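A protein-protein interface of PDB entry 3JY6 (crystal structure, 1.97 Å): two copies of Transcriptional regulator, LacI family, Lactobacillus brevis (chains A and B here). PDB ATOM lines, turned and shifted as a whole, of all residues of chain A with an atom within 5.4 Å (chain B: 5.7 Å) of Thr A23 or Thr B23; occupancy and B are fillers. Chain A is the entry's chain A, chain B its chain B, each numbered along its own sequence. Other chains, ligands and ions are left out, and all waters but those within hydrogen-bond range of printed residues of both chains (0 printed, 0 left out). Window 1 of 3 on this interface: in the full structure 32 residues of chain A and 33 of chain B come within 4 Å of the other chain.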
ATOM      1  N   ILE A  17     -25.071  -6.302 -24.771  1.00  0.00           N
ATOM      2  CA  ILE A  17     -23.901  -6.915 -25.366  1.00  0.00           C
ATOM      3  C   ILE A  17     -22.949  -5.937 -26.056  1.00  0.00           C
ATOM      4  O   ILE A  17     -21.840  -6.320 -26.413  1.00  0.00           O
ATOM      5  CB  ILE A  17     -24.273  -8.045 -26.356  1.00  0.00           C
ATOM      6  CG1 ILE A  17     -25.229  -7.527 -27.428  1.00  0.00           C
ATOM      7  CG2 ILE A  17     -24.861  -9.223 -25.583  1.00  0.00           C
ATOM      8  CD1 ILE A  17     -25.456  -8.532 -28.523  1.00  0.00           C
ATOM      9  N   ASP A  18     -23.366  -4.685 -26.243  1.00  0.00           N
ATOM     10  CA  ASP A  18     -22.475  -3.696 -26.861  1.00  0.00           C
ATOM     11  C   ASP A  18     -21.345  -3.344 -25.908  1.00  0.00           C
ATOM     12  O   ASP A  18     -20.334  -2.789 -26.324  1.00  0.00           O
ATOM     13  CB  ASP A  18     -23.209  -2.405 -27.205  1.00  0.00           C
ATOM     14  CG  ASP A  18     -24.174  -2.572 -28.346  1.00  0.00           C
ATOM     15  OD1 ASP A  18     -23.811  -3.227 -29.359  1.00  0.00           O
ATOM     16  OD2 ASP A  18     -25.298  -2.031 -28.237  1.00  0.00           O
ATOM     17  N   ASP A  19     -21.538  -3.643 -24.626  1.00  0.00           N
ATOM     18  CA  ASP A  19     -20.524  -3.351 -23.622  1.00  0.00           C
ATOM     19  C   ASP A  19     -19.462  -4.439 -23.629  1.00  0.00           C
ATOM     20  O   ASP A  19     -19.765  -5.614 -23.443  1.00  0.00           O
ATOM     21  CB  ASP A  19     -21.128  -3.268 -22.208  1.00  0.00           C
ATOM     22  CG  ASP A  19     -22.221  -2.216 -22.087  1.00  0.00           C
ATOM     23  OD1 ASP A  19     -22.203  -1.245 -22.872  1.00  0.00           O
ATOM     24  OD2 ASP A  19     -23.093  -2.348 -21.195  1.00  0.00           O
ATOM     25  N   TYR A  20     -18.215  -4.039 -23.842  1.00  0.00           N
ATOM     26  CA  TYR A  20     -17.102  -4.978 -23.846  1.00  0.00           C
ATOM     27  C   TYR A  20     -17.089  -5.730 -22.507  1.00  0.00           C
ATOM     28  O   TYR A  20     -16.722  -6.904 -22.449  1.00  0.00           O
ATOM     29  CB  TYR A  20     -15.802  -4.199 -24.044  1.00  0.00           C
ATOM     30  CG  TYR A  20     -14.529  -4.994 -23.873  1.00  0.00           C
ATOM     31  CD1 TYR A  20     -14.011  -5.773 -24.909  1.00  0.00           C
ATOM     32  CD2 TYR A  20     -13.816  -4.934 -22.681  1.00  0.00           C
ATOM     33  CE1 TYR A  20     -12.813  -6.463 -24.760  1.00  0.00           C
ATOM     34  CE2 TYR A  20     -12.620  -5.619 -22.520  1.00  0.00           C
ATOM     35  CZ  TYR A  20     -12.123  -6.380 -23.564  1.00  0.00           C
ATOM     36  OH  TYR A  20     -10.926  -7.050 -23.408  1.00  0.00           O
ATOM     37  N   PHE A  21     -17.493  -5.043 -21.437  1.00  0.00           N
ATOM     38  CA  PHE A  21     -17.542  -5.636 -20.101  1.00  0.00           C
ATOM     39  C   PHE A  21     -18.402  -6.902 -20.092  1.00  0.00           C
ATOM     40  O   PHE A  21     -18.083  -7.876 -19.419  1.00  0.00           O
ATOM     41  CB  PHE A  21     -18.132  -4.638 -19.097  1.00  0.00           C
ATOM     42  CG  PHE A  21     -18.248  -5.174 -17.692  1.00  0.00           C
ATOM     43  CD1 PHE A  21     -17.176  -5.083 -16.806  1.00  0.00           C
ATOM     44  CD2 PHE A  21     -19.430  -5.780 -17.255  1.00  0.00           C
ATOM     45  CE1 PHE A  21     -17.273  -5.582 -15.501  1.00  0.00           C
ATOM     46  CE2 PHE A  21     -19.543  -6.286 -15.954  1.00  0.00           C
ATOM     47  CZ  PHE A  21     -18.459  -6.187 -15.068  1.00  0.00           C
ATOM     48  N   SER A  22     -19.499  -6.870 -20.837  1.00  0.00           N
ATOM     49  CA  SER A  22     -20.416  -7.993 -20.901  1.00  0.00           C
ATOM     50  C   SER A  22     -19.892  -9.174 -21.695  1.00  0.00           C
ATOM     51  O   SER A  22     -19.960 -10.316 -21.243  1.00  0.00           O
ATOM     52  CB  SER A  22     -21.750  -7.547 -21.499  1.00  0.00           C
ATOM     53  OG  SER A  22     -22.433  -6.725 -20.583  1.00  0.00           O
ATOM     54  N   THR A  23     -19.377  -8.905 -22.884  1.00  0.00           N
ATOM     55  CA  THR A  23     -18.873  -9.982 -23.711  1.00  0.00           C
ATOM     56  C   THR A  23     -17.686 -10.666 -23.075  1.00  0.00           C
ATOM     57  O   THR A  23     -17.539 -11.867 -23.226  1.00  0.00           O
ATOM     58  CB  THR A  23     -18.510  -9.487 -25.115  1.00  0.00           C
ATOM     59  OG1 THR A  23     -17.619  -8.367 -25.021  1.00  0.00           O
ATOM     60  CG2 THR A  23     -19.765  -9.087 -25.862  1.00  0.00           C
ATOM     61  N   GLU A  24     -16.849  -9.910 -22.365  1.00  0.00           N
ATOM     62  CA  GLU A  24     -15.681 -10.490 -21.689  1.00  0.00           C
ATOM     63  C   GLU A  24     -16.194 -11.284 -20.505  1.00  0.00           C
ATOM     64  O   GLU A  24     -15.683 -12.360 -20.194  1.00  0.00           O
ATOM     65  CB  GLU A  24     -14.711  -9.413 -21.151  1.00  0.00           C
ATOM     66  CG  GLU A  24     -13.667  -8.942 -22.137  1.00  0.00           C
ATOM     67  CD  GLU A  24     -12.740 -10.066 -22.545  1.00  0.00           C
ATOM     68  OE1 GLU A  24     -11.952 -10.533 -21.696  1.00  0.00           O
ATOM     69  OE2 GLU A  24     -12.805 -10.508 -23.709  1.00  0.00           O
ATOM     70  N   LEU A  25     -17.175 -10.714 -19.813  1.00  0.00           N
ATOM     71  CA  LEU A  25     -17.770 -11.380 -18.661  1.00  0.00           C
ATOM     72  C   LEU A  25     -18.167 -12.771 -19.124  1.00  0.00           C
ATOM     73  O   LEU A  25     -17.812 -13.770 -18.499  1.00  0.00           O
ATOM     74  CB  LEU A  25     -19.021 -10.640 -18.186  1.00  0.00           C
ATOM     75  CG  LEU A  25     -19.562 -11.106 -16.844  1.00  0.00           C
ATOM     76  CD1 LEU A  25     -18.700 -10.500 -15.763  1.00  0.00           C
ATOM     77  CD2 LEU A  25     -20.993 -10.657 -16.663  1.00  0.00           C
ATOM     78  N   PHE A  26     -18.903 -12.818 -20.230  1.00  0.00           N
ATOM     79  CA  PHE A  26     -19.349 -14.085 -20.801  1.00  0.00           C
ATOM     80  C   PHE A  26     -18.201 -15.030 -21.153  1.00  0.00           C
ATOM     81  O   PHE A  26     -18.314 -16.246 -20.969  1.00  0.00           O
ATOM     82  CB  PHE A  26     -20.185 -13.853 -22.049  1.00  0.00           C
ATOM     83  CG  PHE A  26     -20.797 -15.110 -22.599  1.00  0.00           C
ATOM     84  CD1 PHE A  26     -21.796 -15.791 -21.892  1.00  0.00           C
ATOM     85  CD2 PHE A  26     -20.386 -15.612 -23.829  1.00  0.00           C
ATOM     86  CE1 PHE A  26     -22.383 -16.962 -22.410  1.00  0.00           C
ATOM     87  CE2 PHE A  26     -20.963 -16.779 -24.357  1.00  0.00           C
ATOM     88  CZ  PHE A  26     -21.969 -17.457 -23.643  1.00  0.00           C
ATOM     89  N   LYS A  27     -17.115 -14.483 -21.698  1.00  0.00           N
ATOM     90  CA  LYS A  27     -15.962 -15.310 -22.025  1.00  0.00           C
ATOM     91  C   LYS A  27     -15.417 -15.958 -20.754  1.00  0.00           C
ATOM     92  O   LYS A  27     -14.996 -17.107 -20.773  1.00  0.00           O
ATOM     93  CB  LYS A  27     -14.867 -14.469 -22.679  1.00  0.00           C
ATOM     94  CG  LYS A  27     -15.075 -14.218 -24.158  1.00  0.00           C
ATOM     95  CD  LYS A  27     -13.905 -13.424 -24.722  1.00  0.00           C
ATOM     96  CE  LYS A  27     -14.151 -13.025 -26.154  1.00  0.00           C
ATOM     97  NZ  LYS A  27     -14.250 -14.214 -27.034  1.00  0.00           N
ATOM     98  N   GLY A  28     -15.421 -15.210 -19.653  1.00  0.00           N
ATOM     99  CA  GLY A  28     -14.944 -15.740 -18.385  1.00  0.00           C
ATOM    100  C   GLY A  28     -15.823 -16.889 -17.911  1.00  0.00           C
ATOM    101  O   GLY A  28     -15.335 -17.932 -17.481  1.00  0.00           O
ATOM    102  N   LEU A  42     -25.594 -16.837 -23.967  1.00  0.00           N
ATOM    103  CA  LEU A  42     -25.713 -15.395 -23.777  1.00  0.00           C
ATOM    104  C   LEU A  42     -27.034 -14.776 -24.221  1.00  0.00           C
ATOM    105  O   LEU A  42     -27.509 -14.995 -25.343  1.00  0.00           O
ATOM    106  CB  LEU A  42     -24.540 -14.683 -24.465  1.00  0.00           C
ATOM    107  CG  LEU A  42     -24.345 -13.171 -24.246  1.00  0.00           C
ATOM    108  CD1 LEU A  42     -24.287 -12.822 -22.758  1.00  0.00           C
ATOM    109  CD2 LEU A  42     -23.023 -12.758 -24.906  1.00  0.00           C
ATOM    110  N   ILE B  17     -17.476 -12.996 -30.085  1.00  0.00           N
ATOM    111  CA  ILE B  17     -18.386 -12.035 -29.483  1.00  0.00           C
ATOM    112  C   ILE B  17     -17.711 -10.739 -29.094  1.00  0.00           C
ATOM    113  O   ILE B  17     -18.368  -9.797 -28.663  1.00  0.00           O
ATOM    114  CB  ILE B  17     -19.073 -12.598 -28.221  1.00  0.00           C
ATOM    115  CG1 ILE B  17     -18.024 -12.896 -27.144  1.00  0.00           C
ATOM    116  CG2 ILE B  17     -19.846 -13.855 -28.577  1.00  0.00           C
ATOM    117  CD1 ILE B  17     -18.638 -13.281 -25.798  1.00  0.00           C
ATOM    118  N   ASP B  18     -16.398 -10.679 -29.223  1.00  0.00           N
ATOM    119  CA  ASP B  18     -15.709  -9.452 -28.885  1.00  0.00           C
ATOM    120  C   ASP B  18     -15.684  -8.432 -30.041  1.00  0.00           C
ATOM    121  O   ASP B  18     -15.252  -7.296 -29.867  1.00  0.00           O
ATOM    122  CB  ASP B  18     -14.302  -9.773 -28.388  1.00  0.00           C
ATOM    123  CG  ASP B  18     -14.006  -9.107 -27.068  1.00  0.00           C
ATOM    124  OD1 ASP B  18     -13.598  -7.926 -27.097  1.00  0.00           O
ATOM    125  OD2 ASP B  18     -14.195  -9.742 -26.002  1.00  0.00           O
ATOM    126  N   ASP B  19     -16.136  -8.846 -31.220  1.00  0.00           N
ATOM    127  CA  ASP B  19     -16.191  -7.950 -32.379  1.00  0.00           C
ATOM    128  C   ASP B  19     -17.543  -7.225 -32.365  1.00  0.00           C
ATOM    129  O   ASP B  19     -18.576  -7.846 -32.101  1.00  0.00           O
ATOM    130  CB  ASP B  19     -16.111  -8.720 -33.703  1.00  0.00           C
ATOM    131  CG  ASP B  19     -14.853  -9.558 -33.834  1.00  0.00           C
ATOM    132  OD1 ASP B  19     -13.785  -9.143 -33.331  1.00  0.00           O
ATOM    133  OD2 ASP B  19     -14.935 -10.630 -34.473  1.00  0.00           O
ATOM    134  N   TYR B  20     -17.530  -5.928 -32.661  1.00  0.00           N
ATOM    135  CA  TYR B  20     -18.750  -5.122 -32.730  1.00  0.00           C
ATOM    136  C   TYR B  20     -19.645  -5.665 -33.851  1.00  0.00           C
ATOM    137  O   TYR B  20     -20.871  -5.646 -33.732  1.00  0.00           O
ATOM    138  CB  TYR B  20     -18.402  -3.667 -33.035  1.00  0.00           C
ATOM    139  CG  TYR B  20     -19.591  -2.726 -33.148  1.00  0.00           C
ATOM    140  CD1 TYR B  20     -20.282  -2.287 -32.011  1.00  0.00           C
ATOM    141  CD2 TYR B  20     -19.981  -2.225 -34.384  1.00  0.00           C
ATOM    142  CE1 TYR B  20     -21.328  -1.370 -32.110  1.00  0.00           C
ATOM    143  CE2 TYR B  20     -21.024  -1.305 -34.495  1.00  0.00           C
ATOM    144  CZ  TYR B  20     -21.694  -0.882 -33.358  1.00  0.00           C
ATOM    145  OH  TYR B  20     -22.745   0.009 -33.479  1.00  0.00           O
ATOM    146  N   PHE B  21     -19.025  -6.129 -34.938  1.00  0.00           N
ATOM    147  CA  PHE B  21     -19.776  -6.680 -36.060  1.00  0.00           C
ATOM    148  C   PHE B  21     -20.705  -7.778 -35.569  1.00  0.00           C
ATOM    149  O   PHE B  21     -21.858  -7.855 -35.986  1.00  0.00           O
ATOM    150  CB  PHE B  21     -18.843  -7.286 -37.115  1.00  0.00           C
ATOM    151  CG  PHE B  21     -19.564  -8.037 -38.207  1.00  0.00           C
ATOM    152  CD1 PHE B  21     -20.003  -7.382 -39.365  1.00  0.00           C
ATOM    153  CD2 PHE B  21     -19.806  -9.397 -38.073  1.00  0.00           C
ATOM    154  CE1 PHE B  21     -20.679  -8.077 -40.385  1.00  0.00           C
ATOM    155  CE2 PHE B  21     -20.477 -10.108 -39.077  1.00  0.00           C
ATOM    156  CZ  PHE B  21     -20.918  -9.445 -40.242  1.00  0.00           C
ATOM    157  N   SER B  22     -20.182  -8.637 -34.697  1.00  0.00           N
ATOM    158  CA  SER B  22     -20.939  -9.764 -34.150  1.00  0.00           C
ATOM    159  C   SER B  22     -22.064  -9.413 -33.177  1.00  0.00           C
ATOM    160  O   SER B  22     -23.156  -9.989 -33.242  1.00  0.00           O
ATOM    161  CB  SER B  22     -19.983 -10.742 -33.465  1.00  0.00           C
ATOM    162  OG  SER B  22     -19.157 -11.358 -34.434  1.00  0.00           O
ATOM    163  N   THR B  23     -21.798  -8.480 -32.274  1.00  0.00           N
ATOM    164  CA  THR B  23     -22.804  -8.096 -31.300  1.00  0.00           C
ATOM    165  C   THR B  23     -23.913  -7.312 -31.995  1.00  0.00           C
ATOM    166  O   THR B  23     -25.079  -7.428 -31.618  1.00  0.00           O
ATOM    167  CB  THR B  23     -22.194  -7.257 -30.155  1.00  0.00           C
ATOM    168  OG1 THR B  23     -21.642  -6.048 -30.683  1.00  0.00           O
ATOM    169  CG2 THR B  23     -21.095  -8.038 -29.446  1.00  0.00           C
ATOM    170  N   GLU B  24     -23.552  -6.527 -33.015  1.00  0.00           N
ATOM    171  CA  GLU B  24     -24.529  -5.749 -33.773  1.00  0.00           C
ATOM    172  C   GLU B  24     -25.354  -6.668 -34.668  1.00  0.00           C
ATOM    173  O   GLU B  24     -26.557  -6.462 -34.856  1.00  0.00           O
ATOM    174  CB  GLU B  24     -23.848  -4.693 -34.645  1.00  0.00           C
ATOM    175  CG  GLU B  24     -23.603  -3.385 -33.956  1.00  0.00           C
ATOM    176  CD  GLU B  24     -24.883  -2.738 -33.455  1.00  0.00           C
ATOM    177  OE1 GLU B  24     -25.741  -2.372 -34.281  1.00  0.00           O
ATOM    178  OE2 GLU B  24     -25.037  -2.591 -32.228  1.00  0.00           O
ATOM    179  N   LEU B  25     -24.704  -7.676 -35.233  1.00  0.00           N
ATOM    180  CA  LEU B  25     -25.412  -8.627 -36.075  1.00  0.00           C
ATOM    181  C   LEU B  25     -26.449  -9.321 -35.201  1.00  0.00           C
ATOM    182  O   LEU B  25     -27.615  -9.452 -35.587  1.00  0.00           O
ATOM    183  CB  LEU B  25     -24.450  -9.661 -36.654  1.00  0.00           C
ATOM    184  CG  LEU B  25     -25.050 -10.722 -37.574  1.00  0.00           C
ATOM    185  CD1 LEU B  25     -24.314 -10.727 -38.899  1.00  0.00           C
ATOM    186  CD2 LEU B  25     -24.952 -12.066 -36.895  1.00  0.00           C
ATOM    187  N   PHE B  26     -26.036  -9.746 -34.010  1.00  0.00           N
ATOM    188  CA  PHE B  26     -26.967 -10.415 -33.111  1.00  0.00           C
ATOM    189  C   PHE B  26     -28.169  -9.538 -32.758  1.00  0.00           C
ATOM    190  O   PHE B  26     -29.296 -10.034 -32.654  1.00  0.00           O
ATOM    191  CB  PHE B  26     -26.282 -10.865 -31.822  1.00  0.00           C
ATOM    192  CG  PHE B  26     -27.197 -11.630 -30.897  1.00  0.00           C
ATOM    193  CD1 PHE B  26     -27.672 -12.893 -31.249  1.00  0.00           C
ATOM    194  CD2 PHE B  26     -27.658 -11.050 -29.720  1.00  0.00           C
ATOM    195  CE1 PHE B  26     -28.605 -13.570 -30.443  1.00  0.00           C
ATOM    196  CE2 PHE B  26     -28.596 -11.720 -28.900  1.00  0.00           C
ATOM    197  CZ  PHE B  26     -29.069 -12.978 -29.265  1.00  0.00           C
ATOM    198  N   LYS B  27     -27.934  -8.243 -32.560  1.00  0.00           N
ATOM    199  CA  LYS B  27     -29.026  -7.333 -32.234  1.00  0.00           C
ATOM    200  C   LYS B  27     -30.016  -7.258 -33.400  1.00  0.00           C
ATOM    201  O   LYS B  27     -31.207  -7.022 -33.195  1.00  0.00           O
ATOM    202  CB  LYS B  27     -28.486  -5.941 -31.886  1.00  0.00           C
ATOM    203  CG  LYS B  27     -27.912  -5.859 -30.479  1.00  0.00           C
ATOM    204  CD  LYS B  27     -27.357  -4.480 -30.174  1.00  0.00           C
ATOM    205  CE  LYS B  27     -26.872  -4.384 -28.732  1.00  0.00           C
ATOM    206  NZ  LYS B  27     -28.005  -4.457 -27.774  1.00  0.00           N
ATOM    207  N   GLY B  28     -29.516  -7.475 -34.617  1.00  0.00           N
ATOM    208  CA  GLY B  28     -30.372  -7.468 -35.789  1.00  0.00           C
ATOM    209  C   GLY B  28     -31.247  -8.717 -35.837  1.00  0.00           C
ATOM    210  O   GLY B  28     -32.450  -8.619 -36.113  1.00  0.00           O
ATOM    211  N   LEU B  42     -27.139 -16.204 -28.050  1.00  0.00           N
ATOM    212  CA  LEU B  42     -25.794 -16.028 -28.574  1.00  0.00           C
ATOM    213  C   LEU B  42     -24.724 -16.972 -28.026  1.00  0.00           C
ATOM    214  O   LEU B  42     -24.670 -17.245 -26.823  1.00  0.00           O
ATOM    215  CB  LEU B  42     -25.390 -14.566 -28.363  1.00  0.00           C
ATOM    216  CG  LEU B  42     -24.137 -13.964 -28.984  1.00  0.00           C
ATOM    217  CD1 LEU B  42     -24.108 -14.149 -30.491  1.00  0.00           C
ATOM    218  CD2 LEU B  42     -24.124 -12.477 -28.647  1.00  0.00           C
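Of the 13 printed residues of chain B, 7 touch a printed residue of chain A.
Printed residues of chain B that touch a printed residue of chain A: Ile B17, Asp B18, Thr B23, Glu B24, Phe B26, Lys B27 and Leu B42.
Hydrophobic or aromatic side chains of chain A that line the printed part of chain B: Ile A17, Tyr A20, Phe A26 and Leu A42.
Among the printed residues, Asp or Glu carboxylates within 4 Å of a Lys or Arg side-chain nitrogen of the other chain: Asp A18 with Lys B27.
Ile A17 touches Thr B23 (CD1 to O, 3.3 Å).
Ile A17 touches Phe B26.
Ile A17 touches Lys B27 (CG1 to CE, 3.8 Å).
Tyr A20 touches Asp B18 (CE1 to OD1, 2.9 Å).
CD1 of Ile B17 touches O of Thr A23, 3.1 Å away.
OD2 of Asp B18 touches OG1 of Thr A23 (3.8 Å).
Thr A23 touches Thr B23 (CG2 to CG2, 3.96 Å).
Phe A26 touches Ile B17.
Lys A27 touches Ile B17.
Asp B18 touches Lys A27 (OD2 to CE, 3.3 Å).
The side-chain amino group (NZ) of Lys B27 lies within salt-bridge range of the side-chain carboxylate (OD2) of Asp A18, 3.7 Å away.
O of Leu A42 lies within hydrogen-bond range of N of Leu B42 (3.0 Å).
The side-chain carboxylate of Asp A18 lies close to the side-chain carboxylate of Glu B24 (3.2 Å).
The side-chain carboxylate of Glu A24 sits close to the side-chain carboxylate of Asp B18.
The backbone carbonyl oxygen (O) of Tyr A20 is in hydrogen-bond range of the side-chain hydroxyl (OG1) of Thr A23 (3.1 Å).
O of Tyr B20 lies within hydrogen-bond range of OG1 of Thr B23, at 3.2 Å.
Ile A17 touches Phe B26, and with the chains exchanged Phe A26 touches Ile B17.
Asp A18 touches Thr B23, and with the chains exchanged Thr A23 touches Asp B18.
Tyr A20 touches Asp B18, but with the chains exchanged Asp A18 does not touch Tyr B20 (4.1 Å).
Leu B42 touches its own counterpart, Leu A42.
Of the printed residues of chain B, Tyr A20 touches Asp B18 (2.9 Å).
Thr A23 touches three residues of chain B.
Printed residues of chain B within 4 Å of Lys A27: Ile B17 (3.999 Å) and Asp B18 (3.3 Å).
Of the printed residues of chain B, Leu A42 touches Leu B42 (3.0 Å).
Tyr B20 touches none of the printed residues of chain A.
Phe B21 touches none of the printed residues of chain A.
Thr B23 touches just these residues of chain A: Ile A17 (3.3 Å), Asp A18 (3.8 Å) and Thr A23 (3.96 Å).
Of the printed residues of chain A, Glu B24 touches Asp A18 (3.2 Å).
Of the printed residues of chain A, Lys B27 touches Ile A17 (3.8 Å) and Asp A18 (2.9 Å).
The nearest printed residue of chain A that does not touch Thr B23 is Asp A19 (6.5 Å).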
